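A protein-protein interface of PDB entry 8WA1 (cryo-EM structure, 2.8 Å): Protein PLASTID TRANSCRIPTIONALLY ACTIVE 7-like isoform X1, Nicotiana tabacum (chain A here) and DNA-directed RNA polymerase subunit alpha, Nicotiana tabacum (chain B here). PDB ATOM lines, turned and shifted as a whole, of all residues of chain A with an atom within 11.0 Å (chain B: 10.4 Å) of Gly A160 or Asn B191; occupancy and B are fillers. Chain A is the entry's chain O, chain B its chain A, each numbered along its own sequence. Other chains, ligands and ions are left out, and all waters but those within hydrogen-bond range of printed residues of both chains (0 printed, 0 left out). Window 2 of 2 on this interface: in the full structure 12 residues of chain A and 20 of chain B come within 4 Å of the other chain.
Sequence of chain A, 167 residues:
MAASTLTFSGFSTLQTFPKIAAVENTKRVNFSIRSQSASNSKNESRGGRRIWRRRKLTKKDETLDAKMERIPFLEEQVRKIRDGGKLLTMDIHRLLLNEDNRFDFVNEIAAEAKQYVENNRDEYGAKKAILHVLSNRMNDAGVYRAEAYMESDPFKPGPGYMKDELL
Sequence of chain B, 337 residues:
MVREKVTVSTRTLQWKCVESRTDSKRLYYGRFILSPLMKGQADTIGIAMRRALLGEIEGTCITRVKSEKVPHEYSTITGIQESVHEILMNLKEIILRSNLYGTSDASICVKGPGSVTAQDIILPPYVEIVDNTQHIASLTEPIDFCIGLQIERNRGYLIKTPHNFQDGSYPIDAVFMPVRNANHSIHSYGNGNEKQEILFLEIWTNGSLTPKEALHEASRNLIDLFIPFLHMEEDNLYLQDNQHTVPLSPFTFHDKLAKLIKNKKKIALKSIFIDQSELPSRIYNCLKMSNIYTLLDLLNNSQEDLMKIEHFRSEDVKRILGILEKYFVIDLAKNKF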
ATOM      1  N   LYS A 156     -10.965   1.012   8.147  1.00  0.00           N
ATOM      2  CA  LYS A 156      -9.802   0.324   7.611  1.00  0.00           C
ATOM      3  C   LYS A 156      -9.718   0.544   6.101  1.00  0.00           C
ATOM      4  O   LYS A 156     -10.742   0.479   5.408  1.00  0.00           O
ATOM      5  CB  LYS A 156      -9.874  -1.173   7.926  1.00  0.00           C
ATOM      6  N   PRO A 157      -8.529   0.818   5.560  1.00  0.00           N
ATOM      7  CA  PRO A 157      -8.440   1.061   4.109  1.00  0.00           C
ATOM      8  C   PRO A 157      -8.738  -0.173   3.275  1.00  0.00           C
ATOM      9  O   PRO A 157      -9.544  -0.106   2.336  1.00  0.00           O
ATOM     10  CB  PRO A 157      -6.994   1.544   3.932  1.00  0.00           C
ATOM     11  N   GLY A 158      -8.111  -1.302   3.591  1.00  0.00           N
ATOM     12  CA  GLY A 158      -8.319  -2.525   2.853  1.00  0.00           C
ATOM     13  C   GLY A 158      -7.627  -3.705   3.502  1.00  0.00           C
ATOM     14  O   GLY A 158      -7.012  -3.586   4.567  1.00  0.00           O
ATOM     15  N   PRO A 159      -7.718  -4.875   2.874  1.00  0.00           N
ATOM     16  CA  PRO A 159      -7.036  -6.054   3.415  1.00  0.00           C
ATOM     17  C   PRO A 159      -5.525  -5.898   3.354  1.00  0.00           C
ATOM     18  O   PRO A 159      -4.965  -5.375   2.387  1.00  0.00           O
ATOM     19  CB  PRO A 159      -7.516  -7.192   2.508  1.00  0.00           C
ATOM     20  CG  PRO A 159      -7.909  -6.517   1.235  1.00  0.00           C
ATOM     21  CD  PRO A 159      -8.460  -5.180   1.638  1.00  0.00           C
ATOM     22  N   GLY A 160      -4.865  -6.365   4.410  1.00  0.00           N
ATOM     23  CA  GLY A 160      -3.431  -6.230   4.535  1.00  0.00           C
ATOM     24  C   GLY A 160      -2.954  -4.898   5.067  1.00  0.00           C
ATOM     25  O   GLY A 160      -1.749  -4.739   5.297  1.00  0.00           O
ATOM     26  N   TYR A 161      -3.851  -3.938   5.274  1.00  0.00           N
ATOM     27  CA  TYR A 161      -3.509  -2.634   5.820  1.00  0.00           C
ATOM     28  C   TYR A 161      -3.829  -2.617   7.307  1.00  0.00           C
ATOM     29  O   TYR A 161      -4.972  -2.869   7.704  1.00  0.00           O
ATOM     30  CB  TYR A 161      -4.266  -1.515   5.102  1.00  0.00           C
ATOM     31  CG  TYR A 161      -3.815  -1.281   3.677  1.00  0.00           C
ATOM     32  CD1 TYR A 161      -4.318  -2.048   2.634  1.00  0.00           C
ATOM     33  CD2 TYR A 161      -2.891  -0.289   3.375  1.00  0.00           C
ATOM     34  CE1 TYR A 161      -3.909  -1.837   1.331  1.00  0.00           C
ATOM     35  CE2 TYR A 161      -2.476  -0.071   2.075  1.00  0.00           C
ATOM     36  CZ  TYR A 161      -2.988  -0.847   1.057  1.00  0.00           C
ATOM     37  OH  TYR A 161      -2.580  -0.633  -0.239  1.00  0.00           O
ATOM     38  N   MET A 162      -2.822  -2.319   8.123  1.00  0.00           N
ATOM     39  CA  MET A 162      -2.955  -2.311   9.572  1.00  0.00           C
ATOM     40  C   MET A 162      -2.602  -0.933  10.109  1.00  0.00           C
ATOM     41  O   MET A 162      -1.667  -0.289   9.626  1.00  0.00           O
ATOM     42  CB  MET A 162      -2.054  -3.372  10.214  1.00  0.00           C
ATOM     43  CG  MET A 162      -0.627  -3.358   9.689  1.00  0.00           C
ATOM     44  SD  MET A 162       0.358  -4.752  10.263  1.00  0.00           S
ATOM     45  CE  MET A 162       1.795  -4.599   9.204  1.00  0.00           C
ATOM     46  N   LYS A 163      -3.360  -0.485  11.105  1.00  0.00           N
ATOM     47  CA  LYS A 163      -3.108   0.815  11.705  1.00  0.00           C
ATOM     48  C   LYS A 163      -1.821   0.793  12.523  1.00  0.00           C
ATOM     49  O   LYS A 163      -1.412  -0.242  13.056  1.00  0.00           O
ATOM     50  CB  LYS A 163      -4.289   1.238  12.581  1.00  0.00           C
ATOM     51  CG  LYS A 163      -5.086   0.085  13.181  1.00  0.00           C
ATOM     52  CD  LYS A 163      -4.345  -0.597  14.321  1.00  0.00           C
ATOM     53  CE  LYS A 163      -5.147  -1.762  14.880  1.00  0.00           C
ATOM     54  NZ  LYS A 163      -6.482  -1.329  15.377  1.00  0.00           N
ATOM     55  N   ASP A 164      -1.179   1.953  12.613  1.00  0.00           N
ATOM     56  CA  ASP A 164       0.037   2.132  13.395  1.00  0.00           C
ATOM     57  C   ASP A 164      -0.309   2.943  14.635  1.00  0.00           C
ATOM     58  O   ASP A 164      -0.575   4.145  14.538  1.00  0.00           O
ATOM     59  CB  ASP A 164       1.121   2.835  12.579  1.00  0.00           C
ATOM     60  CG  ASP A 164       1.506   2.067  11.330  1.00  0.00           C
ATOM     61  OD1 ASP A 164       1.413   0.821  11.341  1.00  0.00           O
ATOM     62  OD2 ASP A 164       1.907   2.711  10.338  1.00  0.00           O
ATOM     63  N   SER B 188      -2.784   6.095  10.588  1.00  0.00           N
ATOM     64  CA  SER B 188      -1.846   5.690   9.550  1.00  0.00           C
ATOM     65  C   SER B 188      -1.969   4.191   9.317  1.00  0.00           C
ATOM     66  O   SER B 188      -1.622   3.392  10.194  1.00  0.00           O
ATOM     67  CB  SER B 188      -0.413   6.058   9.937  1.00  0.00           C
ATOM     68  OG  SER B 188       0.501   5.677   8.924  1.00  0.00           O
ATOM     69  N   TYR B 189      -2.458   3.816   8.138  1.00  0.00           N
ATOM     70  CA  TYR B 189      -2.569   2.422   7.730  1.00  0.00           C
ATOM     71  C   TYR B 189      -1.504   2.134   6.683  1.00  0.00           C
ATOM     72  O   TYR B 189      -1.489   2.761   5.620  1.00  0.00           O
ATOM     73  CB  TYR B 189      -3.961   2.116   7.170  1.00  0.00           C
ATOM     74  CG  TYR B 189      -5.083   2.322   8.163  1.00  0.00           C
ATOM     75  CD1 TYR B 189      -5.693   3.562   8.307  1.00  0.00           C
ATOM     76  CD2 TYR B 189      -5.536   1.275   8.954  1.00  0.00           C
ATOM     77  CE1 TYR B 189      -6.719   3.752   9.211  1.00  0.00           C
ATOM     78  CE2 TYR B 189      -6.563   1.457   9.859  1.00  0.00           C
ATOM     79  CZ  TYR B 189      -7.150   2.697   9.984  1.00  0.00           C
ATOM     80  OH  TYR B 189      -8.173   2.886  10.885  1.00  0.00           O
ATOM     81  N   GLY B 190      -0.618   1.188   6.985  1.00  0.00           N
ATOM     82  CA  GLY B 190       0.463   0.866   6.078  1.00  0.00           C
ATOM     83  C   GLY B 190       0.589  -0.612   5.780  1.00  0.00           C
ATOM     84  O   GLY B 190       0.664  -1.437   6.697  1.00  0.00           O
ATOM     85  N   ASN B 191       0.614  -0.958   4.496  1.00  0.00           N
ATOM     86  CA  ASN B 191       0.799  -2.330   4.043  1.00  0.00           C
ATOM     87  C   ASN B 191       2.110  -2.416   3.275  1.00  0.00           C
ATOM     88  O   ASN B 191       2.210  -1.902   2.155  1.00  0.00           O
ATOM     89  CB  ASN B 191      -0.369  -2.783   3.166  1.00  0.00           C
ATOM     90  N   GLY B 192       3.102  -3.069   3.872  1.00  0.00           N
ATOM     91  CA  GLY B 192       4.404  -3.170   3.234  1.00  0.00           C
ATOM     92  C   GLY B 192       5.032  -1.807   3.027  1.00  0.00           C
ATOM     93  O   GLY B 192       5.231  -1.038   3.976  1.00  0.00           O
ATOM     94  N   ASN B 193       5.347  -1.494   1.768  1.00  0.00           N
ATOM     95  CA  ASN B 193       6.003  -0.227   1.462  1.00  0.00           C
ATOM     96  C   ASN B 193       5.024   0.940   1.518  1.00  0.00           C
ATOM     97  O   ASN B 193       5.363   2.016   2.026  1.00  0.00           O
ATOM     98  CB  ASN B 193       6.672  -0.302   0.089  1.00  0.00           C
ATOM     99  CG  ASN B 193       5.705  -0.686  -1.013  1.00  0.00           C
ATOM    100  OD1 ASN B 193       4.743  -1.418  -0.781  1.00  0.00           O
ATOM    101  ND2 ASN B 193       5.956  -0.194  -2.220  1.00  0.00           N
ATOM    102  N   GLU B 194       3.813   0.754   1.000  1.00  0.00           N
ATOM    103  CA  GLU B 194       2.846   1.839   0.956  1.00  0.00           C
ATOM    104  C   GLU B 194       2.309   2.150   2.350  1.00  0.00           C
ATOM    105  O   GLU B 194       2.106   1.258   3.178  1.00  0.00           O
ATOM    106  CB  GLU B 194       1.691   1.487   0.018  1.00  0.00           C
ATOM    107  N   LYS B 195       2.079   3.438   2.602  1.00  0.00           N
ATOM    108  CA  LYS B 195       1.527   3.916   3.863  1.00  0.00           C
ATOM    109  C   LYS B 195       0.460   4.959   3.572  1.00  0.00           C
ATOM    110  O   LYS B 195       0.741   5.976   2.929  1.00  0.00           O
ATOM    111  CB  LYS B 195       2.614   4.513   4.766  1.00  0.00           C
ATOM    112  CG  LYS B 195       3.631   3.505   5.274  1.00  0.00           C
ATOM    113  CD  LYS B 195       4.463   4.081   6.411  1.00  0.00           C
ATOM    114  CE  LYS B 195       3.602   4.365   7.634  1.00  0.00           C
ATOM    115  NZ  LYS B 195       4.408   4.853   8.789  1.00  0.00           N
ATOM    116  N   GLN B 196      -0.756   4.709   4.048  1.00  0.00           N
ATOM    117  CA  GLN B 196      -1.878   5.612   3.846  1.00  0.00           C
ATOM    118  C   GLN B 196      -2.311   6.204   5.180  1.00  0.00           C
ATOM    119  O   GLN B 196      -2.327   5.520   6.208  1.00  0.00           O
ATOM    120  CB  GLN B 196      -3.060   4.890   3.187  1.00  0.00           C
ATOM    121  CG  GLN B 196      -2.713   4.209   1.873  1.00  0.00           C
ATOM    122  CD  GLN B 196      -3.894   3.473   1.272  1.00  0.00           C
ATOM    123  OE1 GLN B 196      -3.778   2.843   0.221  1.00  0.00           O
ATOM    124  NE2 GLN B 196      -5.039   3.548   1.939  1.00  0.00           N
ATOM    125  N   GLU B 197      -2.665   7.486   5.154  1.00  0.00           N
ATOM    126  CA  GLU B 197      -3.101   8.207   6.338  1.00  0.00           C
ATOM    127  C   GLU B 197      -4.545   8.658   6.165  1.00  0.00           C
ATOM    128  O   GLU B 197      -4.998   8.926   5.050  1.00  0.00           O
ATOM    129  CB  GLU B 197      -2.209   9.423   6.613  1.00  0.00           C
ATOM    130  CG  GLU B 197      -0.769   9.075   6.951  1.00  0.00           C
ATOM    131  CD  GLU B 197       0.079  10.303   7.212  1.00  0.00           C
ATOM    132  OE1 GLU B 197      -0.373  11.419   6.881  1.00  0.00           O
ATOM    133  OE2 GLU B 197       1.197  10.154   7.749  1.00  0.00           O
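Of the 10 printed residues of chain B, 6 touch a printed residue of chain A.
Hydrophobic or aromatic side chains of chain B within 4 Å of the printed part of chain A: Tyr B189.
Of the 9 printed residues of chain A, 6 touch a printed residue of chain B.
Among the printed residues, 11 pairs touch across the chains.
O of Met A162 lies within hydrogen-bond range of N of Gly B190 (3.2 Å).
The backbone NH (N) of Asp A164 is in hydrogen-bond range of the backbone carbonyl oxygen (O) of Ser B188, at 2.8 Å.
The side-chain carboxylate of Asp A164 is in salt-bridge range of the side-chain amino group of Lys B195 (3.6 Å).
Among the printed residues, pairs that only touch across the chains: Pro A157 with Gln B196 (3.4 Å), Gly A160 with Asn B191 (3.2 Å), Tyr A161 with Asn B191 (3.6 Å), Tyr A161 with Gln B196 (3.7 Å), Met A162 with Ser B188 (3.7 Å), Met A162 with Tyr B189 (3.4 Å), Lys A163 with Ser B188 (3.3 Å) and Lys A163 with Tyr B189 (3.5 Å).
The backbone carbonyl oxygen of Gln B196 is in hydrogen-bond range of the backbone NH of Tyr B189, 2.6 Å away.
Lys A156 touches none of the printed residues of chain B.
Printed residues of chain B within 4 Å of Pro A157: Gln B196.
No residue of chain B comes within 4 Å of Gly A158.
No residue of chain B comes within 4 Å of Pro A159.
Of chain B, only Asn B191 comes within 4 Å of Gly A160.
Of chain B, only Asn B191 (3.6 Å) and Gln B196 (3.7 Å) come within 4 Å of Tyr A161.
Of chain B, only Ser B188, Tyr B189 and Gly B190 come within 4 Å of Met A162.
Printed residues of chain B within 4 Å of Lys A163: Ser B188 (3.3 Å) and Tyr B189 (3.5 Å).
Of the printed residues of chain B, Asp A164 touches Ser B188 (2.8 Å) and Lys B195 (3.6 Å).
Of the printed residues of chain A, Ser B188 touches Met A162, Lys A163 and Asp A164.
Gly B190 touches one residue of chain A.
Asn B191 touches just these residues of chain A: Gly A160 (3.2 Å) and Tyr A161 (3.6 Å).
Gly B192 touches none of the printed residues of chain A.
No residue of chain A comes within 4 Å of Asn B193.
Of the printed residues of chain A, Gln B196 touches Pro A157 and Tyr A161.
Glu B197 touches none of the printed residues of chain A.
The nearest residue of chain A that does not touch Asn B191 is Met A162 (5.2 Å).
The nearest printed residue of chain A that does not touch Ser B188 is Tyr A161 (7.0 Å).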
